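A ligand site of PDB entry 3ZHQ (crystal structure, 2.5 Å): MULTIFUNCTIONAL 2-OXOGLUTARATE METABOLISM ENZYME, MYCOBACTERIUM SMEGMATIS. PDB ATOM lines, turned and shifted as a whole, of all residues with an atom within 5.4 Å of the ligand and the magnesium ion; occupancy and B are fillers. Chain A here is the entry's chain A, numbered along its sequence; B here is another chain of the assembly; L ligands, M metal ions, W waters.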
ATOM      1  N   HIS A 180     -13.941   3.910 -12.740  1.00  0.00           N
ATOM      2  CA  HIS A 180     -15.000   3.042 -13.217  1.00  0.00           C
ATOM      3  C   HIS A 180     -14.578   1.763 -13.979  1.00  0.00           C
ATOM      4  O   HIS A 180     -15.283   0.764 -13.883  1.00  0.00           O
ATOM      5  CB  HIS A 180     -16.029   3.825 -14.068  1.00  0.00           C
ATOM      6  CG  HIS A 180     -15.503   4.604 -15.247  1.00  0.00           C
ATOM      7  ND1 HIS A 180     -15.537   6.008 -15.251  1.00  0.00           N
ATOM      8  CD2 HIS A 180     -15.100   4.179 -16.473  1.00  0.00           C
ATOM      9  CE1 HIS A 180     -15.116   6.382 -16.454  1.00  0.00           C
ATOM     10  NE2 HIS A 180     -14.840   5.328 -17.226  1.00  0.00           N
ATOM     11  N   ARG A 181     -13.465   1.798 -14.744  1.00  0.00           N
ATOM     12  CA  ARG A 181     -12.993   0.672 -15.566  1.00  0.00           C
ATOM     13  C   ARG A 181     -12.703  -0.607 -14.719  1.00  0.00           C
ATOM     14  O   ARG A 181     -11.752  -0.654 -13.946  1.00  0.00           O
ATOM     15  CB  ARG A 181     -11.762   1.081 -16.402  1.00  0.00           C
ATOM     16  CG  ARG A 181     -11.460   0.106 -17.522  1.00  0.00           C
ATOM     17  CD  ARG A 181     -10.355   0.560 -18.479  1.00  0.00           C
ATOM     18  NE  ARG A 181     -10.580   1.877 -19.091  1.00  0.00           N
ATOM     19  CZ  ARG A 181     -11.429   2.121 -20.083  1.00  0.00           C
ATOM     20  NH1 ARG A 181     -12.166   1.137 -20.599  1.00  0.00           N
ATOM     21  NH2 ARG A 181     -11.541   3.339 -20.578  1.00  0.00           N
ATOM     22  N   SER A 245     -16.872  10.957 -10.551  1.00  0.00           N
ATOM     23  CA  SER A 245     -16.350  10.654 -11.898  1.00  0.00           C
ATOM     24  C   SER A 245     -14.990  11.299 -12.046  1.00  0.00           C
ATOM     25  O   SER A 245     -14.171  10.820 -12.822  1.00  0.00           O
ATOM     26  CB  SER A 245     -17.313  11.117 -12.982  1.00  0.00           C
ATOM     27  OG  SER A 245     -18.351  10.176 -13.224  1.00  0.00           O
ATOM     28  N   HIS A 246     -14.734  12.353 -11.237  1.00  0.00           N
ATOM     29  CA  HIS A 246     -13.482  13.108 -11.138  1.00  0.00           C
ATOM     30  C   HIS A 246     -12.327  12.177 -10.847  1.00  0.00           C
ATOM     31  O   HIS A 246     -12.121  11.766  -9.703  1.00  0.00           O
ATOM     32  CB  HIS A 246     -13.598  14.204 -10.053  1.00  0.00           C
ATOM     33  CG  HIS A 246     -14.501  15.309 -10.459  1.00  0.00           C
ATOM     34  ND1 HIS A 246     -15.799  15.086 -10.823  1.00  0.00           N
ATOM     35  CD2 HIS A 246     -14.240  16.631 -10.580  1.00  0.00           C
ATOM     36  CE1 HIS A 246     -16.300  16.260 -11.150  1.00  0.00           C
ATOM     37  NE2 HIS A 246     -15.395  17.223 -11.023  1.00  0.00           N
ATOM     38  N   LEU A 247     -11.583  11.822 -11.903  1.00  0.00           N
ATOM     39  CA  LEU A 247     -10.456  10.892 -11.843  1.00  0.00           C
ATOM     40  C   LEU A 247      -9.395  11.407 -10.861  1.00  0.00           C
ATOM     41  O   LEU A 247      -9.164  12.612 -10.795  1.00  0.00           O
ATOM     42  CB  LEU A 247      -9.879  10.626 -13.251  1.00  0.00           C
ATOM     43  CG  LEU A 247     -10.857   9.940 -14.282  1.00  0.00           C
ATOM     44  CD1 LEU A 247     -10.428  10.181 -15.724  1.00  0.00           C
ATOM     45  CD2 LEU A 247     -11.035   8.447 -14.001  1.00  0.00           C
ATOM     46  N   GLY A 285      -5.556   5.248 -13.807  1.00  0.00           N
ATOM     47  CA  GLY A 285      -5.434   5.252 -15.263  1.00  0.00           C
ATOM     48  C   GLY A 285      -4.139   5.950 -15.604  1.00  0.00           C
ATOM     49  O   GLY A 285      -3.696   6.835 -14.865  1.00  0.00           O
ATOM     50  N   ASP A 286      -3.507   5.565 -16.708  1.00  0.00           N
ATOM     51  CA  ASP A 286      -2.222   6.136 -17.129  1.00  0.00           C
ATOM     52  C   ASP A 286      -2.297   7.640 -17.416  1.00  0.00           C
ATOM     53  O   ASP A 286      -1.361   8.343 -17.034  1.00  0.00           O
ATOM     54  CB  ASP A 286      -1.667   5.385 -18.360  1.00  0.00           C
ATOM     55  CG  ASP A 286      -2.569   5.385 -19.582  1.00  0.00           C
ATOM     56  OD1 ASP A 286      -3.670   4.797 -19.507  1.00  0.00           O
ATOM     57  OD2 ASP A 286      -2.163   5.962 -20.609  1.00  0.00           O
ATOM     58  N   ALA A 287      -3.356   8.159 -18.069  1.00  0.00           N
ATOM     59  CA  ALA A 287      -3.424   9.603 -18.386  1.00  0.00           C
ATOM     60  C   ALA A 287      -3.707  10.414 -17.115  1.00  0.00           C
ATOM     61  O   ALA A 287      -3.073  11.447 -16.890  1.00  0.00           O
ATOM     62  CB  ALA A 287      -4.466   9.892 -19.474  1.00  0.00           C
ATOM     63  N   ALA A 288      -4.630   9.937 -16.263  1.00  0.00           N
ATOM     64  CA  ALA A 288      -5.041  10.605 -15.018  1.00  0.00           C
ATOM     65  C   ALA A 288      -3.898  10.650 -13.973  1.00  0.00           C
ATOM     66  O   ALA A 288      -3.744  11.660 -13.291  1.00  0.00           O
ATOM     67  CB  ALA A 288      -6.258   9.915 -14.440  1.00  0.00           C
ATOM     68  N   PHE A 289      -3.074   9.570 -13.897  1.00  0.00           N
ATOM     69  CA  PHE A 289      -1.945   9.485 -12.956  1.00  0.00           C
ATOM     70  C   PHE A 289      -0.872  10.515 -13.255  1.00  0.00           C
ATOM     71  O   PHE A 289      -0.241  11.053 -12.334  1.00  0.00           O
ATOM     72  CB  PHE A 289      -1.319   8.073 -12.972  1.00  0.00           C
ATOM     73  CG  PHE A 289      -0.524   7.711 -11.736  1.00  0.00           C
ATOM     74  CD1 PHE A 289      -1.156   7.528 -10.518  1.00  0.00           C
ATOM     75  CD2 PHE A 289       0.839   7.525 -11.800  1.00  0.00           C
ATOM     76  CE1 PHE A 289      -0.427   7.171  -9.385  1.00  0.00           C
ATOM     77  CE2 PHE A 289       1.564   7.173 -10.654  1.00  0.00           C
ATOM     78  CZ  PHE A 289       0.929   6.988  -9.460  1.00  0.00           C
ATOM     79  N   GLN A 292      -3.077  14.601 -13.080  1.00  0.00           N
ATOM     80  CA  GLN A 292      -3.826  15.136 -11.947  1.00  0.00           C
ATOM     81  C   GLN A 292      -2.882  15.451 -10.788  1.00  0.00           C
ATOM     82  O   GLN A 292      -2.186  14.559 -10.303  1.00  0.00           O
ATOM     83  CB  GLN A 292      -4.954  14.173 -11.526  1.00  0.00           C
ATOM     84  CG  GLN A 292      -6.130  14.112 -12.511  1.00  0.00           C
ATOM     85  CD  GLN A 292      -6.931  15.411 -12.499  1.00  0.00           C
ATOM     86  OE1 GLN A 292      -7.367  15.885 -11.454  1.00  0.00           O
ATOM     87  NE2 GLN A 292      -7.081  16.041 -13.672  1.00  0.00           N
ATOM     88  N   VAL A 317      -3.513   0.888 -14.442  1.00  0.00           N
ATOM     89  CA  VAL A 317      -4.031   0.155 -15.591  1.00  0.00           C
ATOM     90  C   VAL A 317      -3.592   0.987 -16.811  1.00  0.00           C
ATOM     91  O   VAL A 317      -4.326   1.894 -17.242  1.00  0.00           O
ATOM     92  CB  VAL A 317      -5.562  -0.074 -15.480  1.00  0.00           C
ATOM     93  CG1 VAL A 317      -6.116  -0.759 -16.740  1.00  0.00           C
ATOM     94  CG2 VAL A 317      -5.887  -0.898 -14.210  1.00  0.00           C
ATOM     95  N   ASN A 318      -2.343   0.738 -17.284  1.00  0.00           N
ATOM     96  CA  ASN A 318      -1.724   1.480 -18.395  1.00  0.00           C
ATOM     97  C   ASN A 318      -2.121   0.925 -19.789  1.00  0.00           C
ATOM     98  O   ASN A 318      -1.348   0.204 -20.428  1.00  0.00           O
ATOM     99  CB  ASN A 318      -0.205   1.537 -18.234  1.00  0.00           C
ATOM    100  CG  ASN A 318       0.459   2.566 -19.141  1.00  0.00           C
ATOM    101  OD1 ASN A 318      -0.148   3.164 -20.029  1.00  0.00           O
ATOM    102  ND2 ASN A 318       1.739   2.795 -18.936  1.00  0.00           N
ATOM    103  N   ASN A 319      -3.270   1.347 -20.290  1.00  0.00           N
ATOM    104  CA  ASN A 319      -3.765   0.886 -21.571  1.00  0.00           C
ATOM    105  C   ASN A 319      -3.228   1.776 -22.726  1.00  0.00           C
ATOM    106  O   ASN A 319      -3.625   1.586 -23.893  1.00  0.00           O
ATOM    107  CB  ASN A 319      -5.272   0.800 -21.565  1.00  0.00           C
ATOM    108  CG  ASN A 319      -6.021   2.029 -21.175  1.00  0.00           C
ATOM    109  OD1 ASN A 319      -5.488   3.137 -21.124  1.00  0.00           O
ATOM    110  ND2 ASN A 319      -7.292   1.838 -20.876  1.00  0.00           N
ATOM    111  N   GLN A 320      -2.293   2.705 -22.386  1.00  0.00           N
ATOM    112  CA  GLN A 320      -1.505   3.517 -23.319  1.00  0.00           C
ATOM    113  C   GLN A 320      -2.383   4.419 -24.184  1.00  0.00           C
ATOM    114  O   GLN A 320      -2.036   4.778 -25.318  1.00  0.00           O
ATOM    115  CB  GLN A 320      -0.613   2.588 -24.194  1.00  0.00           C
ATOM    116  CG  GLN A 320       0.154   1.512 -23.383  1.00  0.00           C
ATOM    117  CD  GLN A 320       0.780   0.433 -24.222  1.00  0.00           C
ATOM    118  OE1 GLN A 320       1.441   0.704 -25.220  1.00  0.00           O
ATOM    119  NE2 GLN A 320       0.609  -0.818 -23.821  1.00  0.00           N
ATOM    120  N   ILE A 321      -3.497   4.825 -23.618  1.00  0.00           N
ATOM    121  CA  ILE A 321      -4.474   5.719 -24.266  1.00  0.00           C
ATOM    122  C   ILE A 321      -5.241   6.431 -23.168  1.00  0.00           C
ATOM    123  O   ILE A 321      -5.411   5.885 -22.085  1.00  0.00           O
ATOM    124  CB  ILE A 321      -5.414   4.975 -25.277  1.00  0.00           C
ATOM    125  CG1 ILE A 321      -6.163   5.991 -26.193  1.00  0.00           C
ATOM    126  CG2 ILE A 321      -6.349   3.946 -24.592  1.00  0.00           C
ATOM    127  CD1 ILE A 321      -6.617   5.449 -27.452  1.00  0.00           C
ATOM    128  N   GLY A 322      -5.682   7.639 -23.472  1.00  0.00           N
ATOM    129  CA  GLY A 322      -6.493   8.446 -22.570  1.00  0.00           C
ATOM    130  C   GLY A 322      -7.626   9.039 -23.371  1.00  0.00           C
ATOM    131  O   GLY A 322      -7.493  10.143 -23.917  1.00  0.00           O
ATOM    132  N   PHE A 323      -8.726   8.267 -23.494  1.00  0.00           N
ATOM    133  CA  PHE A 323      -9.930   8.573 -24.276  1.00  0.00           C
ATOM    134  C   PHE A 323      -9.535   8.499 -25.755  1.00  0.00           C
ATOM    135  O   PHE A 323      -9.522   7.402 -26.310  1.00  0.00           O
ATOM    136  CB  PHE A 323     -10.558   9.918 -23.837  1.00  0.00           C
ATOM    137  CG  PHE A 323     -12.035  10.097 -24.142  1.00  0.00           C
ATOM    138  CD1 PHE A 323     -12.452  10.484 -25.415  1.00  0.00           C
ATOM    139  CD2 PHE A 323     -12.991   9.950 -23.154  1.00  0.00           C
ATOM    140  CE1 PHE A 323     -13.810  10.634 -25.701  1.00  0.00           C
ATOM    141  CE2 PHE A 323     -14.337  10.142 -23.436  1.00  0.00           C
ATOM    142  CZ  PHE A 323     -14.746  10.478 -24.720  1.00  0.00           C
ATOM    143  N   ARG A 384      -6.718  -1.170 -24.392  1.00  0.00           N
ATOM    144  CA  ARG A 384      -8.146  -0.930 -24.315  1.00  0.00           C
ATOM    145  C   ARG A 384      -8.820  -1.529 -25.551  1.00  0.00           C
ATOM    146  O   ARG A 384      -8.849  -0.876 -26.606  1.00  0.00           O
ATOM    147  CB  ARG A 384      -8.422   0.582 -24.169  1.00  0.00           C
ATOM    148  CG  ARG A 384      -9.778   0.856 -23.526  1.00  0.00           C
ATOM    149  CD  ARG A 384     -10.254   2.228 -23.876  1.00  0.00           C
ATOM    150  NE  ARG A 384     -10.204   2.498 -25.317  1.00  0.00           N
ATOM    151  CZ  ARG A 384     -10.045   3.712 -25.850  1.00  0.00           C
ATOM    152  NH1 ARG A 384      -9.902   4.769 -25.071  1.00  0.00           N
ATOM    153  NH2 ARG A 384     -10.000   3.859 -27.157  1.00  0.00           N
ATOM    154  N   GLN B 542      -9.391  18.529 -23.210  1.00  0.00           N
ATOM    155  CA  GLN B 542      -9.322  17.069 -23.269  1.00  0.00           C
ATOM    156  C   GLN B 542     -10.082  16.529 -24.469  1.00  0.00           C
ATOM    157  O   GLN B 542     -11.295  16.745 -24.615  1.00  0.00           O
ATOM    158  CB  GLN B 542      -9.853  16.455 -21.974  1.00  0.00           C
ATOM    159  CG  GLN B 542      -8.820  16.495 -20.860  1.00  0.00           C
ATOM    160  CD  GLN B 542      -9.458  16.595 -19.502  1.00  0.00           C
ATOM    161  OE1 GLN B 542     -10.558  16.112 -19.270  1.00  0.00           O
ATOM    162  NE2 GLN B 542      -8.792  17.241 -18.557  1.00  0.00           N
ATOM    163  N   ASP B 543      -9.347  15.863 -25.388  1.00  0.00           N
ATOM    164  CA  ASP B 543      -9.847  15.238 -26.614  1.00  0.00           C
ATOM    165  C   ASP B 543     -10.547  16.250 -27.529  1.00  0.00           C
ATOM    166  O   ASP B 543     -11.468  15.880 -28.261  1.00  0.00           O
ATOM    167  CB  ASP B 543     -10.779  14.070 -26.271  1.00  0.00           C
ATOM    168  CG  ASP B 543     -10.105  13.093 -25.339  1.00  0.00           C
ATOM    169  OD1 ASP B 543      -9.187  12.373 -25.804  1.00  0.00           O
ATOM    170  OD2 ASP B 543     -10.425  13.107 -24.121  1.00  0.00           O
ATOM    171  N   LEU B 591      -4.464  15.357 -19.035  1.00  0.00           N
ATOM    172  CA  LEU B 591      -5.614  15.156 -18.152  1.00  0.00           C
ATOM    173  C   LEU B 591      -5.471  16.071 -16.911  1.00  0.00           C
ATOM    174  O   LEU B 591      -5.374  15.592 -15.776  1.00  0.00           O
ATOM    175  CB  LEU B 591      -5.692  13.682 -17.768  1.00  0.00           C
ATOM    176  CG  LEU B 591      -6.959  13.022 -17.210  1.00  0.00           C
ATOM    177  CD1 LEU B 591      -8.062  13.995 -16.722  1.00  0.00           C
ATOM    178  CD2 LEU B 591      -7.410  11.921 -18.088  1.00  0.00           C
ATOM    179  N   GLU B 593      -6.918  20.086 -15.278  1.00  0.00           N
ATOM    180  CA  GLU B 593      -7.868  21.193 -15.326  1.00  0.00           C
ATOM    181  C   GLU B 593      -7.155  22.426 -14.813  1.00  0.00           C
ATOM    182  O   GLU B 593      -7.033  23.400 -15.534  1.00  0.00           O
ATOM    183  CB  GLU B 593      -9.179  20.902 -14.572  1.00  0.00           C
ATOM    184  CG  GLU B 593     -10.118  19.977 -15.313  1.00  0.00           C
ATOM    185  CD  GLU B 593      -9.843  18.483 -15.195  1.00  0.00           C
ATOM    186  OE1 GLU B 593      -9.324  18.046 -14.138  1.00  0.00           O
ATOM    187  OE2 GLU B 593     -10.222  17.748 -16.123  1.00  0.00           O
ATOM    188  N   GLN B 617     -14.030  18.632 -20.713  1.00  0.00           N
ATOM    189  CA  GLN B 617     -14.570  17.362 -21.235  1.00  0.00           C
ATOM    190  C   GLN B 617     -16.082  17.458 -21.056  1.00  0.00           C
ATOM    191  O   GLN B 617     -16.854  17.338 -22.006  1.00  0.00           O
ATOM    192  CB  GLN B 617     -13.947  16.162 -20.493  1.00  0.00           C
ATOM    193  CG  GLN B 617     -14.459  14.816 -20.976  1.00  0.00           C
ATOM    194  CD  GLN B 617     -13.484  14.101 -21.838  1.00  0.00           C
ATOM    195  OE1 GLN B 617     -13.029  14.601 -22.865  1.00  0.00           O
ATOM    196  NE2 GLN B 617     -13.177  12.892 -21.465  1.00  0.00           N
ATOM    197  N   PHE B 621     -16.143  19.123 -14.657  1.00  0.00           N
ATOM    198  CA  PHE B 621     -14.765  18.898 -14.232  1.00  0.00           C
ATOM    199  C   PHE B 621     -13.962  20.206 -14.076  1.00  0.00           C
ATOM    200  O   PHE B 621     -12.868  20.151 -13.509  1.00  0.00           O
ATOM    201  CB  PHE B 621     -14.072  17.945 -15.218  1.00  0.00           C
ATOM    202  CG  PHE B 621     -14.771  16.617 -15.284  1.00  0.00           C
ATOM    203  CD1 PHE B 621     -14.918  15.839 -14.141  1.00  0.00           C
ATOM    204  CD2 PHE B 621     -15.302  16.154 -16.472  1.00  0.00           C
ATOM    205  CE1 PHE B 621     -15.586  14.613 -14.189  1.00  0.00           C
ATOM    206  CE2 PHE B 621     -15.982  14.936 -16.520  1.00  0.00           C
ATOM    207  CZ  PHE B 621     -16.119  14.172 -15.379  1.00  0.00           C
HETATM  208  N1  LIG L   1     -11.157  15.126 -15.593  1.00  0.00           N
HETATM  209  C1  LIG L   1     -11.373  14.473 -14.459  1.00  0.00           C
HETATM  210  C2  LIG L   1     -10.742  14.945 -13.186  1.00  0.00           C
HETATM  211  N2  LIG L   1     -12.078  13.357 -14.428  1.00  0.00           N
HETATM  212  C3  LIG L   1     -12.696  12.884 -15.529  1.00  0.00           C
HETATM  213  N3  LIG L   1     -13.540  11.807 -15.416  1.00  0.00           N
HETATM  214  C4  LIG L   1     -12.487  13.539 -16.770  1.00  0.00           C
HETATM  215  C5  LIG L   1     -11.698  14.693 -16.741  1.00  0.00           C
HETATM  216  C6  LIG L   1     -13.088  13.066 -18.089  1.00  0.00           C
HETATM  217  N4  LIG L   1     -12.469  11.786 -18.556  1.00  0.00           N
HETATM  218  C7  LIG L   1     -13.135  10.679 -18.444  1.00  0.00           C
HETATM  219  S1  LIG L   1     -12.248   9.323 -19.018  1.00  0.00           S
HETATM  220  C8  LIG L   1     -10.901  10.369 -19.480  1.00  0.00           C
HETATM  221  C9  LIG L   1     -11.247  11.643 -19.104  1.00  0.00           C
HETATM  222  C10 LIG L   1     -10.278  12.764 -19.448  1.00  0.00           C
HETATM  223  C11 LIG L   1      -9.616   9.853 -20.082  1.00  0.00           C
HETATM  224  C12 LIG L   1      -9.124   8.808 -19.086  1.00  0.00           C
HETATM  225  O1  LIG L   1      -7.758   8.443 -19.269  1.00  0.00           O
HETATM  226  P1  LIG L   1      -7.011   7.323 -18.344  1.00  0.00           P
HETATM  227  O2  LIG L   1      -6.606   7.887 -17.030  1.00  0.00           O
HETATM  228  O3  LIG L   1      -5.731   6.809 -19.123  1.00  0.00           O
HETATM  229  O4  LIG L   1      -8.023   6.102 -18.093  1.00  0.00           O
HETATM  230  P2  LIG L   1      -8.614   5.038 -18.983  1.00  0.00           P
HETATM  231  O5  LIG L   1     -10.071   5.495 -19.407  1.00  0.00           O
HETATM  232  O6  LIG L   1      -7.694   4.884 -20.141  1.00  0.00           O
HETATM  233  O7  LIG L   1      -8.677   3.677 -18.138  1.00  0.00           O
HETATM  234 MG    MG M   1      -5.462   4.940 -20.257  1.00  0.00          MG
HETATM  235  O   HOH W   1      -9.162   5.697 -22.529  1.00  0.00           O
HETATM  236  O   HOH W   2      -8.086   6.973 -15.026  1.00  0.00           O
HETATM  237  O   HOH W   3      -5.615   3.659 -18.273  1.00  0.00           O
HETATM  238  O   HOH W   4     -16.094  10.968 -17.096  1.00  0.00           O
HETATM  239  O   HOH W   5      -8.942   4.053 -15.704  1.00  0.00           O
HETATM  240  O   HOH W   6     -11.506   6.645 -21.552  1.00  0.00           O
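OE2 of Glu 593 of chain B sits at hydrogen-bond distance from N1 of the ligand, at 2.8 Å.
The guanidinium group of Arg 181 is in salt-bridge range of an oxygen (O7) of the ligand (2.8 Å).
A nitrogen (N3) of the ligand lies within hydrogen-bond range of the backbone carbonyl oxygen (O) of Ser 245.
N of Leu 247 lies within hydrogen-bond range of N2 of the ligand, at 3.0 Å.
The backbone NH (N) of Ala 288 lies within hydrogen-bond range of an oxygen (O2) of the ligand, at 2.9 Å.
An oxygen (O2) of the ligand lies within hydrogen-bond range of the backbone NH of Ala 287, 3.4 Å away.
The side-chain amide nitrogen of Gln 542 of chain B is in hydrogen-bond range of the side-chain carboxylate of Glu 593 of chain B.
The side-chain carboxylate of Asp 286 sits close to the side-chain amide oxygen of Asn 318.
The side-chain amide nitrogen of Gln 292 sits at hydrogen-bond distance from the side-chain carboxylate of Glu 593 of chain B (3.0 Å).
The backbone carbonyl oxygen of Phe 323 sits at hydrogen-bond distance from the guanidinium group of Arg 384 (2.9 Å).
The side-chain carboxylate (OD2) of Asp 543 of chain B lies close to the side-chain amide oxygen (OE1) of Gln 617 of chain B.
The backbone carbonyl oxygen of Leu 591 of chain B is in hydrogen-bond range of the side-chain amide nitrogen of Gln 292 (2.7 Å).
OE1 of Gln 617 of chain B lies close to O of Gln 542 of chain B (3.3 Å).
N4 of the ligand lies close to NE2 of Gln 617 of chain B (3.2 Å).
His 246 touches the ligand (CA to N2, 3.6 Å).
Gly 285 touches the ligand (CA to O2, 3.4 Å).
Gln 292 touches the ligand.
Gly 322 touches the ligand (CA to O1, 3.5 Å).
N of Phe 323 touches C11 of the ligand (3.9 Å).
OE1 of Gln 542 of chain B touches C5 of the ligand, at 3.1 Å.
Leu 591 of chain B touches the ligand.
Phe 621 of chain B touches the ligand (CZ to N3, 3.5 Å).
Hydrophobic or aromatic side chains that line the ligand: Leu 247, Ala 287, Ala 288, Phe 323, Leu 591 of chain B and Phe 621 of chain B.
Three residues have an atom within 4 Å of the magnesium ion: Asp 286, Asn 319 and Ile 321.
The nearest printed residue that does not touch the magnesium ion is Gly 322 (4.2 Å).
The magnesium ion is bound by OD1 of Asp 286, OD1 of Asn 319, O of Ile 321, O3 of the ligand, O6 of the ligand and water W3.
The magnesium ion has six donor atoms within binding distance.
Water W3 lies within hydrogen-bond range of O of Val 317, O7 of the ligand and N of Asp 286.
Water W2 lies within hydrogen-bond range of an oxygen (O2) of the ligand and the backbone NH (N) of Gly 285.
Water W6 lies within hydrogen-bond range of an oxygen (O5) of the ligand (2.8 Å) and the guanidinium group of Arg 181 (3.4 Å).
Water W1 lies within hydrogen-bond range of N of Phe 323 (2.8 Å), NH1 of Arg 384 (2.8 Å) and O5 of the ligand (3.3 Å).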
